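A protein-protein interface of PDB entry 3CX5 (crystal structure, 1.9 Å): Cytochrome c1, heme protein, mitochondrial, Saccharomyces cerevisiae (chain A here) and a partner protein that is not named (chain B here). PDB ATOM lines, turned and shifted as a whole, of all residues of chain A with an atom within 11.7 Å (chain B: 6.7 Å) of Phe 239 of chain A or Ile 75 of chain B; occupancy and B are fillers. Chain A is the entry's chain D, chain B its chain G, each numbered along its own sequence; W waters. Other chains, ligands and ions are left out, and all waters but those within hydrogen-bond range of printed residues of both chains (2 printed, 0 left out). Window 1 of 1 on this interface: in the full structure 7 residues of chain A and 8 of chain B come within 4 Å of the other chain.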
ATOM      1  N   TRP A 231     -41.259  10.965  20.945  1.00  0.00           N
ATOM      2  CA  TRP A 231     -40.250  10.046  21.462  1.00  0.00           C
ATOM      3  C   TRP A 231     -38.867  10.178  20.820  1.00  0.00           C
ATOM      4  O   TRP A 231     -37.912   9.571  21.296  1.00  0.00           O
ATOM      5  CB  TRP A 231     -40.725   8.605  21.271  1.00  0.00           C
ATOM      6  CG  TRP A 231     -41.620   8.108  22.356  1.00  0.00           C
ATOM      7  CD1 TRP A 231     -42.934   8.419  22.547  1.00  0.00           C
ATOM      8  CD2 TRP A 231     -41.270   7.180  23.386  1.00  0.00           C
ATOM      9  NE1 TRP A 231     -43.430   7.730  23.629  1.00  0.00           N
ATOM     10  CE2 TRP A 231     -42.429   6.964  24.164  1.00  0.00           C
ATOM     11  CE3 TRP A 231     -40.087   6.510  23.730  1.00  0.00           C
ATOM     12  CZ2 TRP A 231     -42.444   6.100  25.266  1.00  0.00           C
ATOM     13  CZ3 TRP A 231     -40.098   5.650  24.828  1.00  0.00           C
ATOM     14  CH2 TRP A 231     -41.273   5.455  25.581  1.00  0.00           C
ATOM     15  N   ALA A 232     -38.756  10.978  19.763  1.00  0.00           N
ATOM     16  CA  ALA A 232     -37.494  11.137  19.035  1.00  0.00           C
ATOM     17  C   ALA A 232     -36.284  11.507  19.883  1.00  0.00           C
ATOM     18  O   ALA A 232     -35.167  11.064  19.595  1.00  0.00           O
ATOM     19  CB  ALA A 232     -37.668  12.135  17.878  1.00  0.00           C
ATOM     20  N   GLY A 233     -36.501  12.319  20.916  1.00  0.00           N
ATOM     21  CA  GLY A 233     -35.415  12.715  21.791  1.00  0.00           C
ATOM     22  C   GLY A 233     -34.906  11.555  22.625  1.00  0.00           C
ATOM     23  O   GLY A 233     -33.698  11.397  22.794  1.00  0.00           O
ATOM     24  N   ILE A 234     -35.827  10.739  23.143  1.00  0.00           N
ATOM     25  CA  ILE A 234     -35.479   9.582  23.968  1.00  0.00           C
ATOM     26  C   ILE A 234     -34.874   8.441  23.131  1.00  0.00           C
ATOM     27  O   ILE A 234     -33.895   7.808  23.530  1.00  0.00           O
ATOM     28  CB  ILE A 234     -36.741   9.033  24.720  1.00  0.00           C
ATOM     29  CG1 ILE A 234     -37.293  10.084  25.695  1.00  0.00           C
ATOM     30  CG2 ILE A 234     -36.421   7.732  25.443  1.00  0.00           C
ATOM     31  CD1 ILE A 234     -36.289  10.578  26.728  1.00  0.00           C
ATOM     32  N   LYS A 235     -35.461   8.193  21.968  1.00  0.00           N
ATOM     33  CA  LYS A 235     -35.018   7.122  21.083  1.00  0.00           C
ATOM     34  C   LYS A 235     -33.589   7.242  20.562  1.00  0.00           C
ATOM     35  O   LYS A 235     -32.903   6.239  20.409  1.00  0.00           O
ATOM     36  CB  LYS A 235     -35.978   7.001  19.901  1.00  0.00           C
ATOM     37  CG  LYS A 235     -37.340   6.437  20.260  1.00  0.00           C
ATOM     38  CD  LYS A 235     -37.329   4.916  20.240  1.00  0.00           C
ATOM     39  CE  LYS A 235     -38.724   4.356  20.470  1.00  0.00           C
ATOM     40  NZ  LYS A 235     -38.768   2.886  20.253  1.00  0.00           N
ATOM     41  N   THR A 236     -33.146   8.470  20.308  1.00  0.00           N
ATOM     42  CA  THR A 236     -31.812   8.710  19.768  1.00  0.00           C
ATOM     43  C   THR A 236     -30.799   9.140  20.824  1.00  0.00           C
ATOM     44  O   THR A 236     -29.667   9.516  20.510  1.00  0.00           O
ATOM     45  CB  THR A 236     -31.884   9.749  18.634  1.00  0.00           C
ATOM     46  OG1 THR A 236     -32.397  10.984  19.144  1.00  0.00           O
ATOM     47  CG2 THR A 236     -32.818   9.255  17.529  1.00  0.00           C
ATOM     48  N   ARG A 237     -31.225   9.054  22.081  1.00  0.00           N
ATOM     49  CA  ARG A 237     -30.427   9.409  23.251  1.00  0.00           C
ATOM     50  C   ARG A 237     -29.121   8.606  23.300  1.00  0.00           C
ATOM     51  O   ARG A 237     -29.112   7.413  23.014  1.00  0.00           O
ATOM     52  CB  ARG A 237     -31.274   9.122  24.491  1.00  0.00           C
ATOM     53  CG  ARG A 237     -30.867   9.797  25.764  1.00  0.00           C
ATOM     54  CD  ARG A 237     -32.040   9.777  26.747  1.00  0.00           C
ATOM     55  NE  ARG A 237     -32.602   8.436  26.893  1.00  0.00           N
ATOM     56  CZ  ARG A 237     -33.090   7.944  28.026  1.00  0.00           C
ATOM     57  NH1 ARG A 237     -33.572   6.707  28.054  1.00  0.00           N
ATOM     58  NH2 ARG A 237     -33.107   8.687  29.125  1.00  0.00           N
ATOM     59  N   LYS A 238     -28.024   9.265  23.661  1.00  0.00           N
ATOM     60  CA  LYS A 238     -26.727   8.601  23.743  1.00  0.00           C
ATOM     61  C   LYS A 238     -26.056   8.712  25.105  1.00  0.00           C
ATOM     62  O   LYS A 238     -26.064   9.766  25.730  1.00  0.00           O
ATOM     63  CB  LYS A 238     -25.805   9.103  22.630  1.00  0.00           C
ATOM     64  CG  LYS A 238     -25.961   8.295  21.358  1.00  0.00           C
ATOM     65  CD  LYS A 238     -25.935   9.161  20.125  1.00  0.00           C
ATOM     66  CE  LYS A 238     -26.188   8.308  18.893  1.00  0.00           C
ATOM     67  NZ  LYS A 238     -26.361   9.127  17.665  1.00  0.00           N
ATOM     68  N   PHE A 239     -25.488   7.599  25.562  1.00  0.00           N
ATOM     69  CA  PHE A 239     -24.823   7.540  26.857  1.00  0.00           C
ATOM     70  C   PHE A 239     -23.338   7.205  26.720  1.00  0.00           C
ATOM     71  O   PHE A 239     -22.942   6.455  25.826  1.00  0.00           O
ATOM     72  CB  PHE A 239     -25.477   6.464  27.738  1.00  0.00           C
ATOM     73  CG  PHE A 239     -26.913   6.739  28.083  1.00  0.00           C
ATOM     74  CD1 PHE A 239     -27.939   6.320  27.242  1.00  0.00           C
ATOM     75  CD2 PHE A 239     -27.245   7.415  29.256  1.00  0.00           C
ATOM     76  CE1 PHE A 239     -29.278   6.572  27.563  1.00  0.00           C
ATOM     77  CE2 PHE A 239     -28.576   7.671  29.585  1.00  0.00           C
ATOM     78  CZ  PHE A 239     -29.596   7.249  28.735  1.00  0.00           C
ATOM     79  N   VAL A 240     -22.522   7.775  27.605  1.00  0.00           N
ATOM     80  CA  VAL A 240     -21.088   7.504  27.634  1.00  0.00           C
ATOM     81  C   VAL A 240     -20.692   7.294  29.091  1.00  0.00           C
ATOM     82  O   VAL A 240     -21.197   7.980  29.982  1.00  0.00           O
ATOM     83  CB  VAL A 240     -20.234   8.666  27.058  1.00  0.00           C
ATOM     84  CG1 VAL A 240     -20.563   8.896  25.590  1.00  0.00           C
ATOM     85  CG2 VAL A 240     -20.446   9.938  27.861  1.00  0.00           C
ATOM     86  N   PHE A 241     -19.798   6.344  29.333  1.00  0.00           N
ATOM     87  CA  PHE A 241     -19.350   6.068  30.688  1.00  0.00           C
ATOM     88  C   PHE A 241     -17.859   6.315  30.850  1.00  0.00           C
ATOM     89  O   PHE A 241     -17.044   5.811  30.071  1.00  0.00           O
ATOM     90  CB  PHE A 241     -19.667   4.623  31.074  1.00  0.00           C
ATOM     91  CG  PHE A 241     -19.361   4.292  32.514  1.00  0.00           C
ATOM     92  CD1 PHE A 241     -19.906   5.052  33.554  1.00  0.00           C
ATOM     93  CD2 PHE A 241     -18.533   3.221  32.833  1.00  0.00           C
ATOM     94  CE1 PHE A 241     -19.628   4.748  34.888  1.00  0.00           C
ATOM     95  CE2 PHE A 241     -18.249   2.910  34.164  1.00  0.00           C
ATOM     96  CZ  PHE A 241     -18.799   3.678  35.193  1.00  0.00           C
ATOM     97  N   ASN A 242     -17.518   7.107  31.862  1.00  0.00           N
ATOM     98  CA  ASN A 242     -16.132   7.412  32.199  1.00  0.00           C
ATOM     99  C   ASN A 242     -15.996   7.050  33.670  1.00  0.00           C
ATOM    100  O   ASN A 242     -16.462   7.788  34.535  1.00  0.00           O
ATOM    101  CB  ASN A 242     -15.827   8.900  31.985  1.00  0.00           C
ATOM    102  CG  ASN A 242     -15.694   9.261  30.521  1.00  0.00           C
ATOM    103  OD1 ASN A 242     -14.740   8.851  29.851  1.00  0.00           O
ATOM    104  ND2 ASN A 242     -16.653  10.027  30.009  1.00  0.00           N
ATOM    105  N   PRO A 243     -15.401   5.878  33.968  1.00  0.00           N
ATOM    106  CA  PRO A 243     -15.210   5.405  35.344  1.00  0.00           C
ATOM    107  C   PRO A 243     -14.647   6.496  36.250  1.00  0.00           C
ATOM    108  O   PRO A 243     -13.542   6.981  36.038  1.00  0.00           O
ATOM    109  CB  PRO A 243     -14.222   4.251  35.171  1.00  0.00           C
ATOM    110  CG  PRO A 243     -14.618   3.683  33.839  1.00  0.00           C
ATOM    111  CD  PRO A 243     -14.801   4.937  33.003  1.00  0.00           C
ATOM    112  N   LEU B  42     -25.043  -6.689  29.284  1.00  0.00           N
ATOM    113  CA  LEU B  42     -25.287  -7.103  30.658  1.00  0.00           C
ATOM    114  C   LEU B  42     -24.527  -8.360  31.070  1.00  0.00           C
ATOM    115  O   LEU B  42     -24.174  -9.189  30.225  1.00  0.00           O
ATOM    116  CB  LEU B  42     -26.791  -7.368  30.846  1.00  0.00           C
ATOM    117  CG  LEU B  42     -27.762  -6.196  30.650  1.00  0.00           C
ATOM    118  CD1 LEU B  42     -29.187  -6.725  30.475  1.00  0.00           C
ATOM    119  CD2 LEU B  42     -27.664  -5.237  31.848  1.00  0.00           C
ATOM    120  N   ARG B  70     -22.127  -1.111  37.232  1.00  0.00           N
ATOM    121  CA  ARG B  70     -23.365  -1.877  37.133  1.00  0.00           C
ATOM    122  C   ARG B  70     -24.497  -0.930  36.718  1.00  0.00           C
ATOM    123  O   ARG B  70     -25.344  -1.283  35.894  1.00  0.00           O
ATOM    124  CB  ARG B  70     -23.720  -2.543  38.469  1.00  0.00           C
ATOM    125  CG  ARG B  70     -24.830  -3.593  38.333  1.00  0.00           C
ATOM    126  CD  ARG B  70     -25.461  -3.993  39.665  1.00  0.00           C
ATOM    127  NE  ARG B  70     -26.229  -2.868  40.136  1.00  0.00           N
ATOM    128  CZ  ARG B  70     -27.526  -2.866  40.404  1.00  0.00           C
ATOM    129  NH1 ARG B  70     -28.067  -1.735  40.795  1.00  0.00           N
ATOM    130  NH2 ARG B  70     -28.259  -3.972  40.338  1.00  0.00           N
ATOM    131  N   ALA B  71     -24.485   0.281  37.274  1.00  0.00           N
ATOM    132  CA  ALA B  71     -25.504   1.281  36.963  1.00  0.00           C
ATOM    133  C   ALA B  71     -25.491   1.592  35.469  1.00  0.00           C
ATOM    134  O   ALA B  71     -26.540   1.614  34.829  1.00  0.00           O
ATOM    135  CB  ALA B  71     -25.277   2.568  37.787  1.00  0.00           C
ATOM    136  N   TYR B  72     -24.300   1.820  34.920  1.00  0.00           N
ATOM    137  CA  TYR B  72     -24.160   2.113  33.496  1.00  0.00           C
ATOM    138  C   TYR B  72     -24.683   0.972  32.616  1.00  0.00           C
ATOM    139  O   TYR B  72     -25.418   1.214  31.658  1.00  0.00           O
ATOM    140  CB  TYR B  72     -22.697   2.401  33.140  1.00  0.00           C
ATOM    141  CG  TYR B  72     -22.485   2.609  31.660  1.00  0.00           C
ATOM    142  CD1 TYR B  72     -23.114   3.659  30.990  1.00  0.00           C
ATOM    143  CD2 TYR B  72     -21.696   1.727  30.913  1.00  0.00           C
ATOM    144  CE1 TYR B  72     -22.970   3.828  29.619  1.00  0.00           C
ATOM    145  CE2 TYR B  72     -21.545   1.887  29.531  1.00  0.00           C
ATOM    146  CZ  TYR B  72     -22.187   2.941  28.895  1.00  0.00           C
ATOM    147  OH  TYR B  72     -22.044   3.117  27.535  1.00  0.00           O
ATOM    148  N   ARG B  73     -24.317  -0.266  32.947  1.00  0.00           N
ATOM    149  CA  ARG B  73     -24.763  -1.415  32.164  1.00  0.00           C
ATOM    150  C   ARG B  73     -26.289  -1.515  32.150  1.00  0.00           C
ATOM    151  O   ARG B  73     -26.890  -1.786  31.110  1.00  0.00           O
ATOM    152  CB  ARG B  73     -24.124  -2.719  32.672  1.00  0.00           C
ATOM    153  CG  ARG B  73     -22.589  -2.774  32.499  1.00  0.00           C
ATOM    154  CD  ARG B  73     -22.041  -4.197  32.685  1.00  0.00           C
ATOM    155  NE  ARG B  73     -22.365  -4.755  33.997  1.00  0.00           N
ATOM    156  CZ  ARG B  73     -21.659  -4.533  35.102  1.00  0.00           C
ATOM    157  NH1 ARG B  73     -22.040  -5.072  36.252  1.00  0.00           N
ATOM    158  NH2 ARG B  73     -20.551  -3.805  35.055  1.00  0.00           N
ATOM    159  N   ILE B  74     -26.915  -1.260  33.294  1.00  0.00           N
ATOM    160  CA  ILE B  74     -28.375  -1.306  33.389  1.00  0.00           C
ATOM    161  C   ILE B  74     -29.044  -0.219  32.533  1.00  0.00           C
ATOM    162  O   ILE B  74     -29.947  -0.510  31.732  1.00  0.00           O
ATOM    163  CB  ILE B  74     -28.810  -1.222  34.865  1.00  0.00           C
ATOM    164  CG1 ILE B  74     -28.450  -2.551  35.549  1.00  0.00           C
ATOM    165  CG2 ILE B  74     -30.314  -0.891  34.990  1.00  0.00           C
ATOM    166  CD1 ILE B  74     -28.646  -2.573  37.034  1.00  0.00           C
ATOM    167  N   ILE B  75     -28.561   1.016  32.651  1.00  0.00           N
ATOM    168  CA  ILE B  75     -29.120   2.132  31.883  1.00  0.00           C
ATOM    169  C   ILE B  75     -28.940   1.909  30.384  1.00  0.00           C
ATOM    170  O   ILE B  75     -29.885   2.050  29.603  1.00  0.00           O
ATOM    171  CB  ILE B  75     -28.479   3.477  32.303  1.00  0.00           C
ATOM    172  CG1 ILE B  75     -28.878   3.810  33.749  1.00  0.00           C
ATOM    173  CG2 ILE B  75     -28.939   4.604  31.370  1.00  0.00           C
ATOM    174  CD1 ILE B  75     -28.144   4.991  34.336  1.00  0.00           C
ATOM    175  N   ARG B  76     -27.722   1.546  29.992  1.00  0.00           N
ATOM    176  CA  ARG B  76     -27.397   1.283  28.594  1.00  0.00           C
ATOM    177  C   ARG B  76     -28.294   0.176  28.027  1.00  0.00           C
ATOM    178  O   ARG B  76     -28.786   0.282  26.904  1.00  0.00           O
ATOM    179  CB  ARG B  76     -25.922   0.900  28.484  1.00  0.00           C
ATOM    180  CG  ARG B  76     -25.495   0.337  27.142  1.00  0.00           C
ATOM    181  CD  ARG B  76     -24.605  -0.860  27.385  1.00  0.00           C
ATOM    182  NE  ARG B  76     -23.199  -0.567  27.198  1.00  0.00           N
ATOM    183  CZ  ARG B  76     -22.205  -1.347  27.610  1.00  0.00           C
ATOM    184  NH1 ARG B  76     -20.956  -0.986  27.364  1.00  0.00           N
ATOM    185  NH2 ARG B  76     -22.447  -2.443  28.317  1.00  0.00           N
ATOM    186  N   ALA B  77     -28.535  -0.864  28.823  1.00  0.00           N
ATOM    187  CA  ALA B  77     -29.375  -1.975  28.402  1.00  0.00           C
ATOM    188  C   ALA B  77     -30.826  -1.531  28.178  1.00  0.00           C
ATOM    189  O   ALA B  77     -31.460  -1.971  27.215  1.00  0.00           O
ATOM    190  CB  ALA B  77     -29.309  -3.101  29.425  1.00  0.00           C
ATOM    191  N   HIS B  78     -31.344  -0.654  29.052  1.00  0.00           N
ATOM    192  CA  HIS B  78     -32.713  -0.155  28.906  1.00  0.00           C
ATOM    193  C   HIS B  78     -32.833   0.660  27.618  1.00  0.00           C
ATOM    194  O   HIS B  78     -33.814   0.530  26.880  1.00  0.00           O
ATOM    195  CB  HIS B  78     -33.140   0.706  30.114  1.00  0.00           C
ATOM    196  CG  HIS B  78     -33.640  -0.092  31.278  1.00  0.00           C
ATOM    197  ND1 HIS B  78     -32.997  -0.119  32.497  1.00  0.00           N
ATOM    198  CD2 HIS B  78     -34.701  -0.927  31.395  1.00  0.00           C
ATOM    199  CE1 HIS B  78     -33.635  -0.942  33.313  1.00  0.00           C
ATOM    200  NE2 HIS B  78     -34.671  -1.445  32.668  1.00  0.00           N
ATOM    201  N   GLN B  79     -31.811   1.468  27.341  1.00  0.00           N
ATOM    202  CA  GLN B  79     -31.785   2.304  26.144  1.00  0.00           C
ATOM    203  C   GLN B  79     -31.757   1.455  24.876  1.00  0.00           C
ATOM    204  O   GLN B  79     -32.462   1.753  23.904  1.00  0.00           O
ATOM    205  CB  GLN B  79     -30.567   3.238  26.160  1.00  0.00           C
ATOM    206  CG  GLN B  79     -30.464   4.156  24.932  1.00  0.00           C
ATOM    207  CD  GLN B  79     -31.669   5.075  24.784  1.00  0.00           C
ATOM    208  OE1 GLN B  79     -32.234   5.534  25.775  1.00  0.00           O
ATOM    209  NE2 GLN B  79     -32.065   5.349  23.541  1.00  0.00           N
ATOM    210  N   THR B  80     -30.950   0.397  24.895  1.00  0.00           N
ATOM    211  CA  THR B  80     -30.831  -0.492  23.744  1.00  0.00           C
ATOM    212  C   THR B  80     -32.152  -1.232  23.518  1.00  0.00           C
ATOM    213  O   THR B  80     -32.617  -1.362  22.389  1.00  0.00           O
ATOM    214  CB  THR B  80     -29.668  -1.505  23.926  1.00  0.00           C
ATOM    215  OG1 THR B  80     -28.477  -0.803  24.303  1.00  0.00           O
ATOM    216  CG2 THR B  80     -29.382  -2.224  22.629  1.00  0.00           C
HETATM  217  O   HOH W   1     -30.149   5.508  21.444  1.00  0.00           O
HETATM  218  O   HOH W   2     -18.887   4.485  27.222  1.00  0.00           O
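The side-chain amide nitrogen (NE2) of Gln 79 of chain B is in hydrogen-bond range of the backbone carbonyl oxygen (O) of Ile 234 of chain A (3.1 Å).
The side-chain amide nitrogen of Gln 79 of chain B sits at hydrogen-bond distance from the backbone carbonyl oxygen of Lys 235 of chain A.
The side-chain amide oxygen of Gln 79 of chain B is in hydrogen-bond range of the guanidinium group of Arg 237 of chain A (2.9 Å).
O of Phe 239 of chain A touches OH of Tyr 72 of chain B, at 3.9 Å.
Phe 239 of chain A touches Ile 75 of chain B (CE2 to CG2, 3.6 Å).
CE1 of Phe 239 of chain A touches OE1 of Gln 79 of chain B, at 3.6 Å.
CB of Phe 241 of chain A touches CG of Tyr 72 of chain B (3.5 Å).
Along chain B the printed residues that touch a printed residue of chain A span positions 72 to 79.
Hydrophobic or aromatic side chains of chain A that line the printed part of chain B: Phe 239 and Phe 241.
Of the printed residues of chain B, Ile 234 of chain A touches Gln 79 (3.1 Å).
Of the printed residues of chain B, Lys 235 of chain A touches Gln 79 (3.4 Å).
Of the printed residues of chain B, Arg 237 of chain A touches Gln 79.
Phe 239 of chain A touches three residues of chain B.
Of the printed residues of chain B, Phe 241 of chain A touches Tyr 72 (3.5 Å).
Pro 243 of chain A touches none of the printed residues of chain B.
No residue of chain A comes within 4 Å of Ala 71 of chain B.
No residue of chain A comes within 4 Å of Ile 74 of chain B.
His 78 of chain B touches none of the printed residues of chain A.
The nearest residue of chain B that does not touch Phe 239 of chain A is Arg 76 of chain B (5.2 Å).
The nearest residue of chain A that does not touch Ile 75 of chain B is Arg 237 of chain A (6.1 Å).
Water W1 lies within hydrogen-bond range of O of Arg 237 of chain A, NE2 of Gln 79 of chain B and O of Lys 235 of chain A.
Water W2 lies within hydrogen-bond range of the backbone NH (N) of Phe 241 of chain A (3.0 Å) and the side-chain hydroxyl (OH) of Tyr 72 of chain B (3.5 Å).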
